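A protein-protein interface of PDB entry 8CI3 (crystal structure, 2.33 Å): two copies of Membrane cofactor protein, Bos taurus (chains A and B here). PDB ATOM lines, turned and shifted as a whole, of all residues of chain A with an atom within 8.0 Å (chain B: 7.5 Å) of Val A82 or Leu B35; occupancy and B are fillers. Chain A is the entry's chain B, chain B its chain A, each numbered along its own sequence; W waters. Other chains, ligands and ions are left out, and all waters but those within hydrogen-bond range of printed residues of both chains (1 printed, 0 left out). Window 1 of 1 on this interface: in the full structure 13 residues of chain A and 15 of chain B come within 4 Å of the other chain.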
ATOM      1  N   VAL A  79      -5.899 -21.195  33.178  1.00  0.00           N
ATOM      2  CA  VAL A  79      -6.428 -21.743  31.943  1.00  0.00           C
ATOM      3  C   VAL A  79      -5.556 -22.929  31.560  1.00  0.00           C
ATOM      4  O   VAL A  79      -4.330 -22.835  31.593  1.00  0.00           O
ATOM      5  CB  VAL A  79      -6.487 -20.684  30.821  1.00  0.00           C
ATOM      6  CG1 VAL A  79      -5.112 -20.225  30.410  1.00  0.00           C
ATOM      7  CG2 VAL A  79      -7.306 -21.221  29.597  1.00  0.00           C
ATOM      8  N   ILE A  80      -6.196 -24.047  31.211  1.00  0.00           N
ATOM      9  CA  ILE A  80      -5.544 -25.317  30.928  1.00  0.00           C
ATOM     10  C   ILE A  80      -5.798 -25.632  29.459  1.00  0.00           C
ATOM     11  O   ILE A  80      -6.951 -25.805  29.041  1.00  0.00           O
ATOM     12  CB  ILE A  80      -6.067 -26.438  31.839  1.00  0.00           C
ATOM     13  CG1 ILE A  80      -6.022 -25.989  33.291  1.00  0.00           C
ATOM     14  CG2 ILE A  80      -5.279 -27.740  31.671  1.00  0.00           C
ATOM     15  CD1 ILE A  80      -6.552 -27.024  34.251  1.00  0.00           C
ATOM     16  N   LEU A  81      -4.727 -25.654  28.675  1.00  0.00           N
ATOM     17  CA  LEU A  81      -4.756 -26.073  27.284  1.00  0.00           C
ATOM     18  C   LEU A  81      -4.751 -27.588  27.280  1.00  0.00           C
ATOM     19  O   LEU A  81      -3.704 -28.229  27.130  1.00  0.00           O
ATOM     20  CB  LEU A  81      -3.555 -25.511  26.536  1.00  0.00           C
ATOM     21  CG  LEU A  81      -3.671 -24.086  25.997  1.00  0.00           C
ATOM     22  CD1 LEU A  81      -4.045 -23.126  27.116  1.00  0.00           C
ATOM     23  CD2 LEU A  81      -2.366 -23.684  25.329  1.00  0.00           C
ATOM     24  N   VAL A  82      -5.947 -28.164  27.487  1.00  0.00           N
ATOM     25  CA  VAL A  82      -6.091 -29.612  27.641  1.00  0.00           C
ATOM     26  C   VAL A  82      -5.694 -30.357  26.383  1.00  0.00           C
ATOM     27  O   VAL A  82      -5.349 -31.533  26.454  1.00  0.00           O
ATOM     28  CB  VAL A  82      -7.527 -30.003  28.064  1.00  0.00           C
ATOM     29  CG1 VAL A  82      -7.799 -29.569  29.507  1.00  0.00           C
ATOM     30  CG2 VAL A  82      -8.582 -29.424  27.099  1.00  0.00           C
ATOM     31  N   ASN A  83      -5.701 -29.708  25.232  1.00  0.00           N
ATOM     32  CA  ASN A  83      -5.307 -30.377  24.006  1.00  0.00           C
ATOM     33  C   ASN A  83      -3.901 -30.017  23.567  1.00  0.00           C
ATOM     34  O   ASN A  83      -3.472 -30.448  22.491  1.00  0.00           O
ATOM     35  CB  ASN A  83      -6.300 -30.049  22.887  1.00  0.00           C
ATOM     36  CG  ASN A  83      -7.713 -30.437  23.243  1.00  0.00           C
ATOM     37  OD1 ASN A  83      -8.651 -29.679  23.026  1.00  0.00           O
ATOM     38  ND2 ASN A  83      -7.862 -31.614  23.821  1.00  0.00           N
ATOM     39  N   GLY A  84      -3.178 -29.231  24.365  1.00  0.00           N
ATOM     40  CA  GLY A  84      -1.805 -28.954  24.047  1.00  0.00           C
ATOM     41  C   GLY A  84      -1.577 -27.843  23.058  1.00  0.00           C
ATOM     42  O   GLY A  84      -0.443 -27.667  22.613  1.00  0.00           O
ATOM     43  N   SER A  85      -2.607 -27.095  22.687  1.00  0.00           N
ATOM     44  CA  SER A  85      -2.424 -26.016  21.725  1.00  0.00           C
ATOM     45  C   SER A  85      -3.694 -25.177  21.698  1.00  0.00           C
ATOM     46  O   SER A  85      -4.660 -25.458  22.412  1.00  0.00           O
ATOM     47  CB  SER A  85      -2.092 -26.571  20.345  1.00  0.00           C
ATOM     48  OG  SER A  85      -3.215 -26.480  19.516  1.00  0.00           O
ATOM     49  N   SER A  90      -9.693 -27.250  19.123  1.00  0.00           N
ATOM     50  CA  SER A  90      -9.277 -27.547  20.485  1.00  0.00           C
ATOM     51  C   SER A  90     -10.146 -26.777  21.455  1.00  0.00           C
ATOM     52  O   SER A  90     -10.827 -25.825  21.071  1.00  0.00           O
ATOM     53  CB  SER A  90      -7.811 -27.143  20.717  1.00  0.00           C
ATOM     54  OG  SER A  90      -7.048 -27.488  19.584  1.00  0.00           O
ATOM     55  N   GLU A  91     -10.030 -27.131  22.740  1.00  0.00           N
ATOM     56  CA  GLU A  91     -10.718 -26.414  23.807  1.00  0.00           C
ATOM     57  C   GLU A  91      -9.775 -26.125  24.973  1.00  0.00           C
ATOM     58  O   GLU A  91      -8.748 -26.794  25.170  1.00  0.00           O
ATOM     59  CB  GLU A  91     -11.914 -27.203  24.326  1.00  0.00           C
ATOM     60  CG  GLU A  91     -11.527 -28.492  25.047  1.00  0.00           C
ATOM     61  CD  GLU A  91     -12.681 -29.504  25.140  1.00  0.00           C
ATOM     62  OE1 GLU A  91     -13.036 -30.131  24.121  1.00  0.00           O
ATOM     63  OE2 GLU A  91     -13.228 -29.671  26.243  1.00  0.00           O
ATOM     64  N   VAL A  92     -10.169 -25.145  25.790  1.00  0.00           N
ATOM     65  CA  VAL A  92      -9.440 -24.822  27.006  1.00  0.00           C
ATOM     66  C   VAL A  92     -10.404 -24.842  28.176  1.00  0.00           C
ATOM     67  O   VAL A  92     -11.597 -24.527  28.043  1.00  0.00           O
ATOM     68  CB  VAL A  92      -8.716 -23.453  26.911  1.00  0.00           C
ATOM     69  CG1 VAL A  92      -7.849 -23.424  25.686  1.00  0.00           C
ATOM     70  CG2 VAL A  92      -9.749 -22.303  26.875  1.00  0.00           C
ATOM     71  N   HIS A  93      -9.875 -25.227  29.335  1.00  0.00           N
ATOM     72  CA  HIS A  93     -10.649 -25.258  30.570  1.00  0.00           C
ATOM     73  C   HIS A  93     -10.167 -24.170  31.524  1.00  0.00           C
ATOM     74  O   HIS A  93      -8.972 -23.937  31.666  1.00  0.00           O
ATOM     75  CB  HIS A  93     -10.552 -26.627  31.229  1.00  0.00           C
ATOM     76  CG  HIS A  93     -11.162 -27.720  30.404  1.00  0.00           C
ATOM     77  ND1 HIS A  93     -11.242 -29.029  30.830  1.00  0.00           N
ATOM     78  CD2 HIS A  93     -11.719 -27.692  29.170  1.00  0.00           C
ATOM     79  CE1 HIS A  93     -11.813 -29.759  29.890  1.00  0.00           C
ATOM     80  NE2 HIS A  93     -12.102 -28.973  28.870  1.00  0.00           N
ATOM     81  N   TYR A  94     -11.104 -23.484  32.154  1.00  0.00           N
ATOM     82  CA  TYR A  94     -10.796 -22.497  33.164  1.00  0.00           C
ATOM     83  C   TYR A  94     -11.135 -23.048  34.538  1.00  0.00           C
ATOM     84  O   TYR A  94     -12.184 -23.687  34.726  1.00  0.00           O
ATOM     85  CB  TYR A  94     -11.576 -21.219  32.927  1.00  0.00           C
ATOM     86  CG  TYR A  94     -11.090 -20.407  31.778  1.00  0.00           C
ATOM     87  CD1 TYR A  94     -10.054 -19.510  31.947  1.00  0.00           C
ATOM     88  CD2 TYR A  94     -11.690 -20.506  30.519  1.00  0.00           C
ATOM     89  CE1 TYR A  94      -9.609 -18.737  30.897  1.00  0.00           C
ATOM     90  CE2 TYR A  94     -11.253 -19.729  29.465  1.00  0.00           C
ATOM     91  CZ  TYR A  94     -10.203 -18.858  29.668  1.00  0.00           C
ATOM     92  OH  TYR A  94      -9.750 -18.075  28.649  1.00  0.00           O
ATOM     93  N   ILE A 107     -15.434 -23.554  29.801  1.00  0.00           N
ATOM     94  CA  ILE A 107     -14.826 -24.171  28.628  1.00  0.00           C
ATOM     95  C   ILE A 107     -14.952 -23.199  27.470  1.00  0.00           C
ATOM     96  O   ILE A 107     -16.051 -22.713  27.182  1.00  0.00           O
ATOM     97  CB  ILE A 107     -15.478 -25.518  28.248  1.00  0.00           C
ATOM     98  CG1 ILE A 107     -15.567 -26.449  29.463  1.00  0.00           C
ATOM     99  CG2 ILE A 107     -14.702 -26.174  27.069  1.00  0.00           C
ATOM    100  CD1 ILE A 107     -15.993 -27.901  29.113  1.00  0.00           C
ATOM    101  N   SER A 108     -13.851 -22.950  26.774  1.00  0.00           N
ATOM    102  CA  SER A 108     -13.930 -22.175  25.545  1.00  0.00           C
ATOM    103  C   SER A 108     -13.374 -23.021  24.406  1.00  0.00           C
ATOM    104  O   SER A 108     -12.451 -23.811  24.610  1.00  0.00           O
ATOM    105  CB  SER A 108     -13.190 -20.852  25.691  1.00  0.00           C
ATOM    106  OG  SER A 108     -13.668 -19.905  24.759  1.00  0.00           O
ATOM    107  N   SER B  12      -0.303 -28.489  37.735  1.00  0.00           N
ATOM    108  CA  SER B  12       0.649 -29.009  36.764  1.00  0.00           C
ATOM    109  C   SER B  12       0.496 -30.491  36.460  1.00  0.00           C
ATOM    110  O   SER B  12       1.240 -31.004  35.612  1.00  0.00           O
ATOM    111  CB  SER B  12       2.076 -28.782  37.280  1.00  0.00           C
ATOM    112  OG  SER B  12       2.334 -29.693  38.331  1.00  0.00           O
ATOM    113  N   MET B  13      -0.405 -31.194  37.145  1.00  0.00           N
ATOM    114  CA  MET B  13      -0.559 -32.631  37.022  1.00  0.00           C
ATOM    115  C   MET B  13      -2.024 -32.953  36.748  1.00  0.00           C
ATOM    116  O   MET B  13      -2.901 -32.118  36.971  1.00  0.00           O
ATOM    117  CB  MET B  13      -0.133 -33.367  38.299  1.00  0.00           C
ATOM    118  CG  MET B  13       1.187 -32.989  38.877  1.00  0.00           C
ATOM    119  SD  MET B  13       1.416 -33.717  40.514  1.00  0.00           S
ATOM    120  CE  MET B  13       0.594 -32.531  41.555  1.00  0.00           C
ATOM    121  N   LYS B  14      -2.281 -34.178  36.296  1.00  0.00           N
ATOM    122  CA  LYS B  14      -3.620 -34.745  36.158  1.00  0.00           C
ATOM    123  C   LYS B  14      -3.578 -36.224  36.517  1.00  0.00           C
ATOM    124  O   LYS B  14      -2.515 -36.850  36.460  1.00  0.00           O
ATOM    125  CB  LYS B  14      -4.178 -34.588  34.735  1.00  0.00           C
ATOM    126  CG  LYS B  14      -3.254 -35.121  33.652  1.00  0.00           C
ATOM    127  CD  LYS B  14      -3.948 -35.202  32.307  1.00  0.00           C
ATOM    128  CE  LYS B  14      -4.999 -36.339  32.288  1.00  0.00           C
ATOM    129  NZ  LYS B  14      -5.786 -36.408  31.021  1.00  0.00           N
ATOM    130  N   GLU B  32       0.278 -37.515  36.729  1.00  0.00           N
ATOM    131  CA  GLU B  32       1.299 -37.369  35.714  1.00  0.00           C
ATOM    132  C   GLU B  32       1.245 -35.934  35.224  1.00  0.00           C
ATOM    133  O   GLU B  32       0.228 -35.254  35.378  1.00  0.00           O
ATOM    134  CB  GLU B  32       1.074 -38.342  34.553  1.00  0.00           C
ATOM    135  CG  GLU B  32      -0.125 -37.966  33.686  1.00  0.00           C
ATOM    136  CD  GLU B  32      -0.344 -38.934  32.532  1.00  0.00           C
ATOM    137  OE1 GLU B  32       0.436 -39.908  32.434  1.00  0.00           O
ATOM    138  OE2 GLU B  32      -1.290 -38.723  31.727  1.00  0.00           O
ATOM    139  N   CYS B  33       2.332 -35.487  34.605  1.00  0.00           N
ATOM    140  CA  CYS B  33       2.380 -34.112  34.136  1.00  0.00           C
ATOM    141  C   CYS B  33       1.304 -33.876  33.090  1.00  0.00           C
ATOM    142  O   CYS B  33       1.002 -34.751  32.273  1.00  0.00           O
ATOM    143  CB  CYS B  33       3.761 -33.772  33.564  1.00  0.00           C
ATOM    144  SG  CYS B  33       5.125 -33.839  34.784  1.00  0.00           S
ATOM    145  N   ARG B  34       0.690 -32.700  33.158  1.00  0.00           N
ATOM    146  CA  ARG B  34      -0.169 -32.263  32.081  1.00  0.00           C
ATOM    147  C   ARG B  34       0.653 -32.079  30.816  1.00  0.00           C
ATOM    148  O   ARG B  34       1.878 -31.897  30.850  1.00  0.00           O
ATOM    149  CB  ARG B  34      -0.855 -30.940  32.428  1.00  0.00           C
ATOM    150  CG  ARG B  34      -1.722 -30.959  33.660  1.00  0.00           C
ATOM    151  CD  ARG B  34      -2.419 -29.619  33.835  1.00  0.00           C
ATOM    152  NE  ARG B  34      -3.413 -29.695  34.896  1.00  0.00           N
ATOM    153  CZ  ARG B  34      -4.629 -30.234  34.754  1.00  0.00           C
ATOM    154  NH1 ARG B  34      -5.020 -30.749  33.582  1.00  0.00           N
ATOM    155  NH2 ARG B  34      -5.455 -30.263  35.800  1.00  0.00           N
ATOM    156  N   LEU B  35      -0.044 -32.125  29.693  1.00  0.00           N
ATOM    157  CA  LEU B  35       0.501 -31.669  28.426  1.00  0.00           C
ATOM    158  C   LEU B  35       1.148 -30.308  28.603  1.00  0.00           C
ATOM    159  O   LEU B  35       0.558 -29.393  29.193  1.00  0.00           O
ATOM    160  CB  LEU B  35      -0.618 -31.590  27.386  1.00  0.00           C
ATOM    161  CG  LEU B  35      -1.135 -32.967  26.963  1.00  0.00           C
ATOM    162  CD1 LEU B  35      -2.264 -32.834  25.931  1.00  0.00           C
ATOM    163  CD2 LEU B  35       0.067 -33.768  26.407  1.00  0.00           C
ATOM    164  N   GLY B  36       2.376 -30.176  28.098  1.00  0.00           N
ATOM    165  CA  GLY B  36       3.064 -28.925  28.184  1.00  0.00           C
ATOM    166  C   GLY B  36       3.837 -28.693  29.467  1.00  0.00           C
ATOM    167  O   GLY B  36       4.445 -27.626  29.606  1.00  0.00           O
ATOM    168  N   PHE B  37       3.822 -29.645  30.398  1.00  0.00           N
ATOM    169  CA  PHE B  37       4.557 -29.584  31.652  1.00  0.00           C
ATOM    170  C   PHE B  37       5.546 -30.743  31.722  1.00  0.00           C
ATOM    171  O   PHE B  37       5.361 -31.763  31.060  1.00  0.00           O
ATOM    172  CB  PHE B  37       3.608 -29.632  32.861  1.00  0.00           C
ATOM    173  CG  PHE B  37       2.744 -28.421  32.992  1.00  0.00           C
ATOM    174  CD1 PHE B  37       1.650 -28.225  32.136  1.00  0.00           C
ATOM    175  CD2 PHE B  37       3.006 -27.467  33.960  1.00  0.00           C
ATOM    176  CE1 PHE B  37       0.842 -27.098  32.249  1.00  0.00           C
ATOM    177  CE2 PHE B  37       2.187 -26.337  34.071  1.00  0.00           C
ATOM    178  CZ  PHE B  37       1.102 -26.157  33.218  1.00  0.00           C
ATOM    179  N   GLN B  38       6.583 -30.593  32.544  1.00  0.00           N
ATOM    180  CA  GLN B  38       7.603 -31.613  32.737  1.00  0.00           C
ATOM    181  C   GLN B  38       7.832 -31.851  34.221  1.00  0.00           C
ATOM    182  O   GLN B  38       7.566 -30.968  35.045  1.00  0.00           O
ATOM    183  CB  GLN B  38       8.936 -31.212  32.074  1.00  0.00           C
ATOM    184  CG  GLN B  38       9.475 -29.911  32.583  1.00  0.00           C
ATOM    185  CD  GLN B  38      10.675 -29.436  31.812  1.00  0.00           C
ATOM    186  OE1 GLN B  38      10.625 -28.416  31.107  1.00  0.00           O
ATOM    187  NE2 GLN B  38      11.780 -30.159  31.949  1.00  0.00           N
ATOM    188  N   LYS B  65       5.864 -25.829  33.959  1.00  0.00           N
ATOM    189  CA  LYS B  65       5.563 -25.523  32.570  1.00  0.00           C
ATOM    190  C   LYS B  65       6.829 -25.600  31.704  1.00  0.00           C
ATOM    191  O   LYS B  65       7.861 -24.985  32.018  1.00  0.00           O
ATOM    192  CB  LYS B  65       4.892 -24.144  32.498  1.00  0.00           C
ATOM    193  CG  LYS B  65       4.232 -23.841  31.184  1.00  0.00           C
ATOM    194  CD  LYS B  65       3.371 -22.584  31.196  1.00  0.00           C
ATOM    195  CE  LYS B  65       2.282 -22.620  32.244  1.00  0.00           C
ATOM    196  NZ  LYS B  65       1.289 -21.515  32.020  1.00  0.00           N
ATOM    197  N   ARG B  66       6.763 -26.394  30.632  1.00  0.00           N
ATOM    198  CA  ARG B  66       7.869 -26.480  29.694  1.00  0.00           C
ATOM    199  C   ARG B  66       8.100 -25.147  28.983  1.00  0.00           C
ATOM    200  O   ARG B  66       7.236 -24.260  28.955  1.00  0.00           O
ATOM    201  CB  ARG B  66       7.641 -27.564  28.655  1.00  0.00           C
ATOM    202  CG  ARG B  66       7.562 -28.952  29.235  1.00  0.00           C
ATOM    203  CD  ARG B  66       7.150 -30.020  28.191  1.00  0.00           C
ATOM    204  NE  ARG B  66       7.261 -31.356  28.754  1.00  0.00           N
ATOM    205  CZ  ARG B  66       8.313 -32.149  28.596  1.00  0.00           C
ATOM    206  NH1 ARG B  66       9.348 -31.749  27.880  1.00  0.00           N
ATOM    207  NH2 ARG B  66       8.335 -33.336  29.160  1.00  0.00           N
ATOM    208  N   PHE B  88       5.324 -22.802  27.396  1.00  0.00           N
ATOM    209  CA  PHE B  88       4.171 -23.439  26.787  1.00  0.00           C
ATOM    210  C   PHE B  88       2.942 -22.551  26.883  1.00  0.00           C
ATOM    211  O   PHE B  88       2.641 -22.001  27.941  1.00  0.00           O
ATOM    212  CB  PHE B  88       3.902 -24.764  27.496  1.00  0.00           C
ATOM    213  CG  PHE B  88       2.562 -25.375  27.154  1.00  0.00           C
ATOM    214  CD1 PHE B  88       2.330 -25.901  25.894  1.00  0.00           C
ATOM    215  CD2 PHE B  88       1.546 -25.440  28.101  1.00  0.00           C
ATOM    216  CE1 PHE B  88       1.091 -26.462  25.576  1.00  0.00           C
ATOM    217  CE2 PHE B  88       0.326 -25.999  27.788  1.00  0.00           C
ATOM    218  CZ  PHE B  88       0.096 -26.525  26.522  1.00  0.00           C
ATOM    219  N   VAL B 112       2.601 -28.377  22.349  1.00  0.00           N
ATOM    220  CA  VAL B 112       3.042 -29.772  22.422  1.00  0.00           C
ATOM    221  C   VAL B 112       3.328 -30.303  21.022  1.00  0.00           C
ATOM    222  O   VAL B 112       2.481 -30.233  20.124  1.00  0.00           O
ATOM    223  CB  VAL B 112       1.983 -30.637  23.126  1.00  0.00           C
ATOM    224  CG1 VAL B 112       2.311 -32.099  23.009  1.00  0.00           C
ATOM    225  CG2 VAL B 112       1.900 -30.276  24.576  1.00  0.00           C
ATOM    226  N   SER B 114       5.444 -33.651  20.512  1.00  0.00           N
ATOM    227  CA  SER B 114       5.176 -35.042  20.833  1.00  0.00           C
ATOM    228  C   SER B 114       4.843 -35.116  22.318  1.00  0.00           C
ATOM    229  O   SER B 114       4.963 -34.125  23.043  1.00  0.00           O
ATOM    230  CB  SER B 114       6.369 -35.937  20.486  1.00  0.00           C
ATOM    231  OG  SER B 114       6.118 -37.277  20.857  1.00  0.00           O
ATOM    232  N   GLY B 115       4.414 -36.294  22.771  1.00  0.00           N
ATOM    233  CA  GLY B 115       4.045 -36.499  24.163  1.00  0.00           C
ATOM    234  C   GLY B 115       5.011 -35.880  25.155  1.00  0.00           C
ATOM    235  O   GLY B 115       4.600 -35.200  26.101  1.00  0.00           O
ATOM    236  N   THR B 116       6.303 -36.102  24.942  1.00  0.00           N
ATOM    237  CA  THR B 116       7.345 -35.340  25.613  1.00  0.00           C
ATOM    238  C   THR B 116       7.876 -34.305  24.628  1.00  0.00           C
ATOM    239  O   THR B 116       8.378 -34.662  23.555  1.00  0.00           O
ATOM    240  CB  THR B 116       8.476 -36.240  26.111  1.00  0.00           C
ATOM    241  OG1 THR B 116       9.028 -36.977  25.012  1.00  0.00           O
ATOM    242  CG2 THR B 116       7.967 -37.209  27.171  1.00  0.00           C
ATOM    243  N   GLY B 117       7.730 -33.029  24.980  1.00  0.00           N
ATOM    244  CA  GLY B 117       8.306 -31.952  24.203  1.00  0.00           C
ATOM    245  C   GLY B 117       7.315 -30.897  23.764  1.00  0.00           C
ATOM    246  O   GLY B 117       6.178 -31.205  23.378  1.00  0.00           O
ATOM    247  N   VAL B 118       7.733 -29.643  23.847  1.00  0.00           N
ATOM    248  CA  VAL B 118       7.050 -28.542  23.187  1.00  0.00           C
ATOM    249  C   VAL B 118       7.904 -28.104  22.002  1.00  0.00           C
ATOM    250  O   VAL B 118       9.091 -28.415  21.918  1.00  0.00           O
ATOM    251  CB  VAL B 118       6.751 -27.351  24.138  1.00  0.00           C
ATOM    252  CG1 VAL B 118       5.589 -27.693  25.093  1.00  0.00           C
ATOM    253  CG2 VAL B 118       8.019 -26.863  24.920  1.00  0.00           C
HETATM  254  O   HOH W   1      -2.245 -28.853  29.509  1.00  0.00           O
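O of Gly A84 sits at hydrogen-bond distance from N of Val B112 (3.1 Å).
O of Arg B66 sits at hydrogen-bond distance from N of Phe B88 (2.9 Å).
NE of Arg B34 lies within hydrogen-bond range of O of Met B13, at 3.2 Å.
The backbone NH (N) of Ile A80 is in hydrogen-bond range of the backbone carbonyl oxygen (O) of His A93, 2.8 Å away.
The backbone NH of Arg B34 sits at hydrogen-bond distance from the backbone carbonyl oxygen of Ser B12 (3.0 Å).
Ile A80 touches Arg B34.
Leu A81 touches Phe B88.
Leu B35 touches Val A82.
Phe B88 touches Gly A84 (CE1 to O, 3.5 Å).
Of the printed residues of chain B, Ile A80 touches Arg B34.
Of the printed residues of chain B, Leu A81 touches Phe B88.
Val A82 touches just one residue of chain B: Leu B35 (3.4 Å).
Printed residues of chain B within 4 Å of Gly A84: Phe B88 (3.5 Å) and Val B112 (3.1 Å).
Ile A107 touches none of the printed residues of chain B.
Of chain A, only Val A82 (3.4 Å) comes within 4 Å of Leu B35.
Lys B65 touches none of the printed residues of chain A.
The nearest residue of chain B that does not touch Val A82 is Arg B34 (5.1 Å).
The nearest printed residue of chain A that does not touch Leu B35 is Asn A83 (4.03 Å).
Printed residues of chain A that touch a printed residue of chain B: Ile A80, Leu A81, Val A82 and Gly A84.
Among the printed residues, 5 pairs touch across the chains.
Among the printed residues, no Asp or Glu carboxylate lies within 4 Å of a Lys or Arg side-chain nitrogen of the other chain.
No position is printed for both chains.
Of the 5 pairs that touch across the chains among the printed residues, none has its exchanged pair printed and touching as well.
Water W1 lies within hydrogen-bond range of the backbone carbonyl oxygen of Leu A81 (2.9 Å) and the backbone carbonyl oxygen of Leu B35 (2.9 Å).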
